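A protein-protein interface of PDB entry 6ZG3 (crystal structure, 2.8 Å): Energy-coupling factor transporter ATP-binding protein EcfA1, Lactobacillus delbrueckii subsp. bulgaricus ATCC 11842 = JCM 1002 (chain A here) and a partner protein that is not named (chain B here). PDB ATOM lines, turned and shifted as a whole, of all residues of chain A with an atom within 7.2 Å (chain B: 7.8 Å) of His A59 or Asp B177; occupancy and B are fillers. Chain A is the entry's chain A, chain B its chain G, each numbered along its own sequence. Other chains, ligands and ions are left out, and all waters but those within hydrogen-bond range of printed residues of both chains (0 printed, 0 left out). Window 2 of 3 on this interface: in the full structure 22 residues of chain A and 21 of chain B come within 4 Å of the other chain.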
ATOM      1  N   ILE A  57      24.110  25.063  18.706  1.00  0.00           N
ATOM      2  CA  ILE A  57      24.008  25.562  20.070  1.00  0.00           C
ATOM      3  C   ILE A  57      24.229  27.066  20.082  1.00  0.00           C
ATOM      4  O   ILE A  57      24.937  27.615  19.234  1.00  0.00           O
ATOM      5  CB  ILE A  57      25.025  24.884  20.990  1.00  0.00           C
ATOM      6  CG1 ILE A  57      26.432  25.154  20.463  1.00  0.00           C
ATOM      7  CG2 ILE A  57      24.807  23.409  20.996  1.00  0.00           C
ATOM      8  CD1 ILE A  57      27.501  24.710  21.380  1.00  0.00           C
ATOM      9  N   GLY A  58      23.601  27.734  21.035  1.00  0.00           N
ATOM     10  CA  GLY A  58      23.698  29.180  21.104  1.00  0.00           C
ATOM     11  C   GLY A  58      22.911  29.692  22.287  1.00  0.00           C
ATOM     12  O   GLY A  58      22.111  28.969  22.886  1.00  0.00           O
ATOM     13  N   HIS A  59      23.131  30.970  22.602  1.00  0.00           N
ATOM     14  CA  HIS A  59      22.586  31.584  23.810  1.00  0.00           C
ATOM     15  C   HIS A  59      22.008  32.964  23.533  1.00  0.00           C
ATOM     16  O   HIS A  59      22.630  33.767  22.832  1.00  0.00           O
ATOM     17  CB  HIS A  59      23.661  31.700  24.895  1.00  0.00           C
ATOM     18  CG  HIS A  59      23.182  32.364  26.149  1.00  0.00           C
ATOM     19  ND1 HIS A  59      22.185  31.838  26.941  1.00  0.00           N
ATOM     20  CD2 HIS A  59      23.558  33.524  26.738  1.00  0.00           C
ATOM     21  CE1 HIS A  59      21.972  32.644  27.968  1.00  0.00           C
ATOM     22  NE2 HIS A  59      22.794  33.673  27.870  1.00  0.00           N
ATOM     23  N   ASN A  60      20.839  33.250  24.131  1.00  0.00           N
ATOM     24  CA  ASN A  60      20.173  34.553  24.045  1.00  0.00           C
ATOM     25  C   ASN A  60      19.952  34.953  22.591  1.00  0.00           C
ATOM     26  O   ASN A  60      18.825  35.185  22.166  1.00  0.00           O
ATOM     27  CB  ASN A  60      21.010  35.635  24.752  1.00  0.00           C
ATOM     28  CG  ASN A  60      20.684  35.774  26.237  1.00  0.00           C
ATOM     29  OD1 ASN A  60      19.600  35.395  26.689  1.00  0.00           O
ATOM     30  ND2 ASN A  60      21.635  36.324  27.009  1.00  0.00           N
ATOM     31  N   GLY A  61      21.047  35.034  21.838  1.00  0.00           N
ATOM     32  CA  GLY A  61      20.989  35.237  20.410  1.00  0.00           C
ATOM     33  C   GLY A  61      20.130  34.220  19.701  1.00  0.00           C
ATOM     34  O   GLY A  61      19.614  34.502  18.620  1.00  0.00           O
ATOM     35  N   SER A  62      20.047  32.993  20.258  1.00  0.00           N
ATOM     36  CA  SER A  62      19.076  31.953  19.899  1.00  0.00           C
ATOM     37  C   SER A  62      18.641  32.004  18.443  1.00  0.00           C
ATOM     38  O   SER A  62      17.456  31.778  18.160  1.00  0.00           O
ATOM     39  CB  SER A  62      17.808  32.045  20.778  1.00  0.00           C
ATOM     40  OG  SER A  62      17.852  31.226  21.933  1.00  0.00           O
ATOM     41  N   GLY A  63      19.559  32.319  17.523  1.00  0.00           N
ATOM     42  CA  GLY A  63      19.197  32.266  16.117  1.00  0.00           C
ATOM     43  C   GLY A  63      18.835  30.868  15.665  1.00  0.00           C
ATOM     44  O   GLY A  63      18.058  30.711  14.715  1.00  0.00           O
ATOM     45  N   LYS A  64      19.319  29.855  16.392  1.00  0.00           N
ATOM     46  CA  LYS A  64      19.014  28.466  16.091  1.00  0.00           C
ATOM     47  C   LYS A  64      17.524  28.187  16.169  1.00  0.00           C
ATOM     48  O   LYS A  64      17.019  27.349  15.406  1.00  0.00           O
ATOM     49  CB  LYS A  64      19.782  27.543  17.043  1.00  0.00           C
ATOM     50  CG  LYS A  64      20.275  28.197  18.317  1.00  0.00           C
ATOM     51  CD  LYS A  64      20.554  27.169  19.387  1.00  0.00           C
ATOM     52  CE  LYS A  64      19.515  27.242  20.463  1.00  0.00           C
ATOM     53  NZ  LYS A  64      19.333  28.693  20.729  1.00  0.00           N
ATOM     54  N   THR A 219      19.814  22.596  20.063  1.00  0.00           N
ATOM     55  CA  THR A 219      19.662  22.276  21.470  1.00  0.00           C
ATOM     56  C   THR A 219      20.478  23.148  22.398  1.00  0.00           C
ATOM     57  O   THR A 219      21.358  23.910  21.997  1.00  0.00           O
ATOM     58  CB  THR A 219      20.044  20.839  21.748  1.00  0.00           C
ATOM     59  OG1 THR A 219      19.997  20.639  23.157  1.00  0.00           O
ATOM     60  CG2 THR A 219      21.442  20.541  21.249  1.00  0.00           C
ATOM     61  N   HIS A 220      20.125  23.024  23.676  1.00  0.00           N
ATOM     62  CA  HIS A 220      20.894  23.546  24.797  1.00  0.00           C
ATOM     63  C   HIS A 220      21.311  22.436  25.763  1.00  0.00           C
ATOM     64  O   HIS A 220      21.675  22.720  26.907  1.00  0.00           O
ATOM     65  CB  HIS A 220      20.116  24.659  25.518  1.00  0.00           C
ATOM     66  CG  HIS A 220      18.758  24.253  26.040  1.00  0.00           C
ATOM     67  ND1 HIS A 220      18.556  23.154  26.853  1.00  0.00           N
ATOM     68  CD2 HIS A 220      17.542  24.841  25.900  1.00  0.00           C
ATOM     69  CE1 HIS A 220      17.274  23.069  27.171  1.00  0.00           C
ATOM     70  NE2 HIS A 220      16.638  24.084  26.608  1.00  0.00           N
ATOM     71  N   ASP A 221      21.241  21.176  25.335  1.00  0.00           N
ATOM     72  CA  ASP A 221      21.753  20.037  26.102  1.00  0.00           C
ATOM     73  C   ASP A 221      23.179  19.800  25.623  1.00  0.00           C
ATOM     74  O   ASP A 221      23.404  19.176  24.581  1.00  0.00           O
ATOM     75  CB  ASP A 221      20.887  18.796  25.897  1.00  0.00           C
ATOM     76  CG  ASP A 221      21.353  17.589  26.721  1.00  0.00           C
ATOM     77  OD1 ASP A 221      22.240  17.754  27.583  1.00  0.00           O
ATOM     78  OD2 ASP A 221      20.828  16.467  26.499  1.00  0.00           O
ATOM     79  N   VAL A 233      28.268  26.685  16.608  1.00  0.00           N
ATOM     80  CA  VAL A 233      27.979  27.644  17.653  1.00  0.00           C
ATOM     81  C   VAL A 233      27.374  28.875  16.978  1.00  0.00           C
ATOM     82  O   VAL A 233      27.938  29.409  16.015  1.00  0.00           O
ATOM     83  CB  VAL A 233      29.262  27.976  18.436  1.00  0.00           C
ATOM     84  CG1 VAL A 233      28.940  28.609  19.758  1.00  0.00           C
ATOM     85  CG2 VAL A 233      30.084  26.726  18.632  1.00  0.00           C
ATOM     86  N   LEU A 234      26.222  29.318  17.465  1.00  0.00           N
ATOM     87  CA  LEU A 234      25.530  30.471  16.922  1.00  0.00           C
ATOM     88  C   LEU A 234      25.509  31.531  18.005  1.00  0.00           C
ATOM     89  O   LEU A 234      25.158  31.249  19.157  1.00  0.00           O
ATOM     90  CB  LEU A 234      24.104  30.125  16.469  1.00  0.00           C
ATOM     91  CG  LEU A 234      23.764  29.424  15.139  1.00  0.00           C
ATOM     92  CD1 LEU A 234      22.295  29.633  14.756  1.00  0.00           C
ATOM     93  CD2 LEU A 234      24.643  29.906  14.007  1.00  0.00           C
ATOM     94  N   ASP A 235      25.920  32.738  17.634  1.00  0.00           N
ATOM     95  CA  ASP A 235      25.985  33.875  18.537  1.00  0.00           C
ATOM     96  C   ASP A 235      25.361  35.078  17.842  1.00  0.00           C
ATOM     97  O   ASP A 235      25.822  35.485  16.769  1.00  0.00           O
ATOM     98  CB  ASP A 235      27.433  34.151  18.938  1.00  0.00           C
ATOM     99  CG  ASP A 235      27.580  35.380  19.810  1.00  0.00           C
ATOM    100  OD1 ASP A 235      27.124  35.368  20.987  1.00  0.00           O
ATOM    101  OD2 ASP A 235      28.151  36.366  19.289  1.00  0.00           O
ATOM    102  N   ASP A 236      24.300  35.623  18.442  1.00  0.00           N
ATOM    103  CA  ASP A 236      23.572  36.782  17.921  1.00  0.00           C
ATOM    104  C   ASP A 236      23.266  36.669  16.428  1.00  0.00           C
ATOM    105  O   ASP A 236      23.488  37.604  15.651  1.00  0.00           O
ATOM    106  CB  ASP A 236      24.333  38.068  18.218  1.00  0.00           C
ATOM    107  CG  ASP A 236      23.841  38.741  19.463  1.00  0.00           C
ATOM    108  OD1 ASP A 236      23.138  38.076  20.259  1.00  0.00           O
ATOM    109  OD2 ASP A 236      24.137  39.938  19.634  1.00  0.00           O
ATOM    110  N   GLY A 237      22.720  35.524  16.024  1.00  0.00           N
ATOM    111  CA  GLY A 237      22.352  35.385  14.632  1.00  0.00           C
ATOM    112  C   GLY A 237      23.509  35.223  13.675  1.00  0.00           C
ATOM    113  O   GLY A 237      23.352  35.464  12.482  1.00  0.00           O
ATOM    114  N   LEU A 255      33.059  30.147  24.598  1.00  0.00           N
ATOM    115  CA  LEU A 255      31.704  29.772  24.965  1.00  0.00           C
ATOM    116  C   LEU A 255      31.237  30.528  26.204  1.00  0.00           C
ATOM    117  O   LEU A 255      30.091  30.975  26.266  1.00  0.00           O
ATOM    118  CB  LEU A 255      31.634  28.265  25.191  1.00  0.00           C
ATOM    119  CG  LEU A 255      32.125  27.411  24.005  1.00  0.00           C
ATOM    120  CD1 LEU A 255      32.052  25.934  24.332  1.00  0.00           C
ATOM    121  CD2 LEU A 255      31.361  27.710  22.717  1.00  0.00           C
ATOM    122  N   LYS A 256      32.103  30.689  27.214  1.00  0.00           N
ATOM    123  CA  LYS A 256      31.674  31.441  28.388  1.00  0.00           C
ATOM    124  C   LYS A 256      31.252  32.849  28.003  1.00  0.00           C
ATOM    125  O   LYS A 256      30.265  33.368  28.542  1.00  0.00           O
ATOM    126  CB  LYS A 256      32.745  31.492  29.472  1.00  0.00           C
ATOM    127  CG  LYS A 256      32.287  32.221  30.739  1.00  0.00           C
ATOM    128  CD  LYS A 256      33.388  32.271  31.765  1.00  0.00           C
ATOM    129  CE  LYS A 256      33.446  31.002  32.583  1.00  0.00           C
ATOM    130  NZ  LYS A 256      34.516  31.060  33.623  1.00  0.00           N
ATOM    131  N   ARG A 257      32.006  33.516  27.121  1.00  0.00           N
ATOM    132  CA  ARG A 257      31.614  34.867  26.704  1.00  0.00           C
ATOM    133  C   ARG A 257      30.271  34.839  25.993  1.00  0.00           C
ATOM    134  O   ARG A 257      29.418  35.682  26.270  1.00  0.00           O
ATOM    135  CB  ARG A 257      32.670  35.540  25.829  1.00  0.00           C
ATOM    136  CG  ARG A 257      32.249  36.971  25.353  1.00  0.00           C
ATOM    137  CD  ARG A 257      31.654  37.838  26.488  1.00  0.00           C
ATOM    138  NE  ARG A 257      31.199  39.178  26.073  1.00  0.00           N
ATOM    139  CZ  ARG A 257      29.945  39.501  25.724  1.00  0.00           C
ATOM    140  NH1 ARG A 257      28.978  38.586  25.714  1.00  0.00           N
ATOM    141  NH2 ARG A 257      29.650  40.753  25.378  1.00  0.00           N
ATOM    142  N   ILE A 258      30.070  33.892  25.054  1.00  0.00           N
ATOM    143  CA  ILE A 258      28.754  33.783  24.409  1.00  0.00           C
ATOM    144  C   ILE A 258      27.652  33.569  25.438  1.00  0.00           C
ATOM    145  O   ILE A 258      26.510  34.006  25.239  1.00  0.00           O
ATOM    146  CB  ILE A 258      28.697  32.612  23.412  1.00  0.00           C
ATOM    147  CG1 ILE A 258      29.842  32.615  22.413  1.00  0.00           C
ATOM    148  CG2 ILE A 258      27.349  32.569  22.694  1.00  0.00           C
ATOM    149  CD1 ILE A 258      29.928  31.292  21.705  1.00  0.00           C
ATOM    150  N   GLY A 259      27.974  32.940  26.564  1.00  0.00           N
ATOM    151  CA  GLY A 259      26.993  32.552  27.553  1.00  0.00           C
ATOM    152  C   GLY A 259      26.758  31.064  27.598  1.00  0.00           C
ATOM    153  O   GLY A 259      25.923  30.604  28.378  1.00  0.00           O
ATOM    154  N   LEU A 260      27.451  30.302  26.767  1.00  0.00           N
ATOM    155  CA  LEU A 260      27.321  28.858  26.775  1.00  0.00           C
ATOM    156  C   LEU A 260      28.165  28.227  27.878  1.00  0.00           C
ATOM    157  O   LEU A 260      29.221  28.736  28.254  1.00  0.00           O
ATOM    158  CB  LEU A 260      27.771  28.286  25.435  1.00  0.00           C
ATOM    159  CG  LEU A 260      27.067  28.878  24.239  1.00  0.00           C
ATOM    160  CD1 LEU A 260      27.705  28.330  22.984  1.00  0.00           C
ATOM    161  CD2 LEU A 260      25.608  28.540  24.353  1.00  0.00           C
ATOM    162  N   ASP A 261      27.707  27.082  28.365  1.00  0.00           N
ATOM    163  CA  ASP A 261      28.506  26.227  29.227  1.00  0.00           C
ATOM    164  C   ASP A 261      29.214  25.185  28.358  1.00  0.00           C
ATOM    165  O   ASP A 261      29.288  25.325  27.135  1.00  0.00           O
ATOM    166  CB  ASP A 261      27.630  25.575  30.297  1.00  0.00           C
ATOM    167  CG  ASP A 261      28.425  25.116  31.504  1.00  0.00           C
ATOM    168  OD1 ASP A 261      29.606  24.704  31.340  1.00  0.00           O
ATOM    169  OD2 ASP A 261      27.853  25.128  32.614  1.00  0.00           O
ATOM    170  N   ARG B 153      10.391  34.394  34.361  1.00  0.00           N
ATOM    171  CA  ARG B 153      10.840  35.236  35.453  1.00  0.00           C
ATOM    172  C   ARG B 153       9.691  36.079  35.995  1.00  0.00           C
ATOM    173  O   ARG B 153       9.583  36.279  37.213  1.00  0.00           O
ATOM    174  CB  ARG B 153      11.992  36.103  34.983  1.00  0.00           C
ATOM    175  CG  ARG B 153      13.241  35.321  34.654  1.00  0.00           C
ATOM    176  CD  ARG B 153      14.127  36.210  33.821  1.00  0.00           C
ATOM    177  NE  ARG B 153      15.523  35.797  33.806  1.00  0.00           N
ATOM    178  CZ  ARG B 153      16.445  36.389  33.054  1.00  0.00           C
ATOM    179  NH1 ARG B 153      16.096  37.420  32.281  1.00  0.00           N
ATOM    180  NH2 ARG B 153      17.704  35.956  33.075  1.00  0.00           N
ATOM    181  N   ALA B 173      13.149  25.306  36.457  1.00  0.00           N
ATOM    182  CA  ALA B 173      14.133  25.509  35.397  1.00  0.00           C
ATOM    183  C   ALA B 173      13.868  24.673  34.138  1.00  0.00           C
ATOM    184  O   ALA B 173      14.792  24.434  33.359  1.00  0.00           O
ATOM    185  CB  ALA B 173      15.538  25.232  35.932  1.00  0.00           C
ATOM    186  N   ALA B 174      12.625  24.251  33.905  1.00  0.00           N
ATOM    187  CA  ALA B 174      12.297  23.443  32.736  1.00  0.00           C
ATOM    188  C   ALA B 174      12.406  24.248  31.445  1.00  0.00           C
ATOM    189  O   ALA B 174      11.672  25.218  31.246  1.00  0.00           O
ATOM    190  CB  ALA B 174      10.888  22.882  32.883  1.00  0.00           C
ATOM    191  N   GLY B 175      13.273  23.814  30.535  1.00  0.00           N
ATOM    192  CA  GLY B 175      13.443  24.488  29.262  1.00  0.00           C
ATOM    193  C   GLY B 175      14.513  25.563  29.228  1.00  0.00           C
ATOM    194  O   GLY B 175      14.852  26.050  28.135  1.00  0.00           O
ATOM    195  N   LEU B 176      15.061  25.932  30.383  1.00  0.00           N
ATOM    196  CA  LEU B 176      16.079  26.963  30.457  1.00  0.00           C
ATOM    197  C   LEU B 176      17.439  26.397  30.068  1.00  0.00           C
ATOM    198  O   LEU B 176      17.802  25.295  30.478  1.00  0.00           O
ATOM    199  CB  LEU B 176      16.119  27.516  31.873  1.00  0.00           C
ATOM    200  CG  LEU B 176      14.797  28.187  32.198  1.00  0.00           C
ATOM    201  CD1 LEU B 176      14.708  28.534  33.656  1.00  0.00           C
ATOM    202  CD2 LEU B 176      14.696  29.427  31.346  1.00  0.00           C
ATOM    203  N   ASP B 177      18.195  27.170  29.276  1.00  0.00           N
ATOM    204  CA  ASP B 177      19.501  26.749  28.789  1.00  0.00           C
ATOM    205  C   ASP B 177      20.464  26.692  29.973  1.00  0.00           C
ATOM    206  O   ASP B 177      20.140  27.189  31.047  1.00  0.00           O
ATOM    207  CB  ASP B 177      19.989  27.701  27.696  1.00  0.00           C
ATOM    208  CG  ASP B 177      20.439  29.025  28.235  1.00  0.00           C
ATOM    209  OD1 ASP B 177      19.705  29.605  29.057  1.00  0.00           O
ATOM    210  OD2 ASP B 177      21.533  29.482  27.829  1.00  0.00           O
ATOM    211  N   PRO B 178      21.657  26.078  29.809  1.00  0.00           N
ATOM    212  CA  PRO B 178      22.555  25.859  30.955  1.00  0.00           C
ATOM    213  C   PRO B 178      22.733  27.023  31.923  1.00  0.00           C
ATOM    214  O   PRO B 178      22.661  26.855  33.146  1.00  0.00           O
ATOM    215  CB  PRO B 178      23.885  25.537  30.269  1.00  0.00           C
ATOM    216  CG  PRO B 178      23.490  24.831  29.025  1.00  0.00           C
ATOM    217  CD  PRO B 178      22.179  25.418  28.593  1.00  0.00           C
ATOM    218  N   MET B 179      22.960  28.216  31.380  1.00  0.00           N
ATOM    219  CA  MET B 179      23.233  29.385  32.210  1.00  0.00           C
ATOM    220  C   MET B 179      21.975  29.950  32.873  1.00  0.00           C
ATOM    221  O   MET B 179      22.041  30.427  34.014  1.00  0.00           O
ATOM    222  CB  MET B 179      23.949  30.443  31.369  1.00  0.00           C
ATOM    223  CG  MET B 179      24.114  31.790  32.039  1.00  0.00           C
ATOM    224  SD  MET B 179      25.265  32.861  31.156  1.00  0.00           S
ATOM    225  CE  MET B 179      26.838  32.088  31.593  1.00  0.00           C
ATOM    226  N   GLY B 180      20.839  29.955  32.168  1.00  0.00           N
ATOM    227  CA  GLY B 180      19.605  30.466  32.763  1.00  0.00           C
ATOM    228  C   GLY B 180      19.160  29.678  33.983  1.00  0.00           C
ATOM    229  O   GLY B 180      18.699  30.250  34.972  1.00  0.00           O
ATOM    230  N   ARG B 181      19.306  28.350  33.930  1.00  0.00           N
ATOM    231  CA  ARG B 181      19.015  27.506  35.087  1.00  0.00           C
ATOM    232  C   ARG B 181      19.947  27.831  36.246  1.00  0.00           C
ATOM    233  O   ARG B 181      19.535  27.827  37.414  1.00  0.00           O
ATOM    234  CB  ARG B 181      19.104  26.027  34.677  1.00  0.00           C
ATOM    235  CG  ARG B 181      19.266  25.018  35.814  1.00  0.00           C
ATOM    236  CD  ARG B 181      19.279  23.545  35.336  1.00  0.00           C
ATOM    237  NE  ARG B 181      18.049  22.841  35.715  1.00  0.00           N
ATOM    238  CZ  ARG B 181      17.523  21.800  35.069  1.00  0.00           C
ATOM    239  NH1 ARG B 181      18.105  21.317  33.978  1.00  0.00           N
ATOM    240  NH2 ARG B 181      16.404  21.241  35.522  1.00  0.00           N
ATOM    241  N   LEU B 182      21.210  28.115  35.940  1.00  0.00           N
ATOM    242  CA  LEU B 182      22.137  28.551  36.972  1.00  0.00           C
ATOM    243  C   LEU B 182      21.660  29.847  37.608  1.00  0.00           C
ATOM    244  O   LEU B 182      21.683  29.986  38.835  1.00  0.00           O
ATOM    245  CB  LEU B 182      23.520  28.724  36.362  1.00  0.00           C
ATOM    246  CG  LEU B 182      24.599  29.241  37.293  1.00  0.00           C
ATOM    247  CD1 LEU B 182      24.779  28.347  38.527  1.00  0.00           C
ATOM    248  CD2 LEU B 182      25.891  29.396  36.513  1.00  0.00           C
ATOM    249  N   GLU B 183      21.216  30.809  36.791  1.00  0.00           N
ATOM    250  CA  GLU B 183      20.660  32.042  37.353  1.00  0.00           C
ATOM    251  C   GLU B 183      19.479  31.739  38.265  1.00  0.00           C
ATOM    252  O   GLU B 183      19.327  32.348  39.329  1.00  0.00           O
ATOM    253  CB  GLU B 183      20.202  33.009  36.257  1.00  0.00           C
ATOM    254  CG  GLU B 183      21.238  33.636  35.346  1.00  0.00           C
ATOM    255  CD  GLU B 183      20.626  34.791  34.548  1.00  0.00           C
ATOM    256  OE1 GLU B 183      20.051  34.521  33.464  1.00  0.00           O
ATOM    257  OE2 GLU B 183      20.682  35.958  35.024  1.00  0.00           O
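Among the printed residues, pairs that only touch across the chains: His A220 with Asp B177 (3.7 Å), His A220 with Pro B178 (3.2 Å) and Asp A261 with Pro B178 (3.7 Å).
ND1 of His A59 lies within hydrogen-bond range of OD2 of Asp B177, at 2.6 Å.
A ring nitrogen (NE2) of His A220 sits at hydrogen-bond distance from the backbone carbonyl oxygen (O) of Gly B175 (3.1 Å).
The backbone carbonyl oxygen (O) of Gly A259 sits close to the side-chain sulfur (SD) of Met B179, at 3.6 Å.
NE2 of His A59 lies within hydrogen-bond range of ND2 of Asn A60 (3.0 Å).
The side-chain carboxylate of Asp B177 is in hydrogen-bond range of the backbone NH of Gly B180.
Of the 23 printed residues of chain A, 4 touch a printed residue of chain B.
Hydrophobic or aromatic side chains of chain A that line the printed part of chain B: His A59 and His A220.
Of the 12 printed residues of chain B, 4 touch a printed residue of chain A.
Among the printed residues, 6 pairs touch across the chains.
Among the printed residues, no Asp or Glu carboxylate lies within 4 Å of a Lys or Arg side-chain nitrogen of the other chain.
Of chain A, only His A59 (2.6 Å) and His A220 (3.7 Å) come within 4 Å of Asp B177.
No residue of chain B comes within 4 Å of Gly A58.
Of the printed residues of chain A, Gly B175 touches His A220.
Of the printed residues of chain B, Asp A261 touches Pro B178.
Printed residues of chain A within 4 Å of Met B179: Gly A259.
Lys A256 touches none of the printed residues of chain B.
Asp A221 touches none of the printed residues of chain B.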
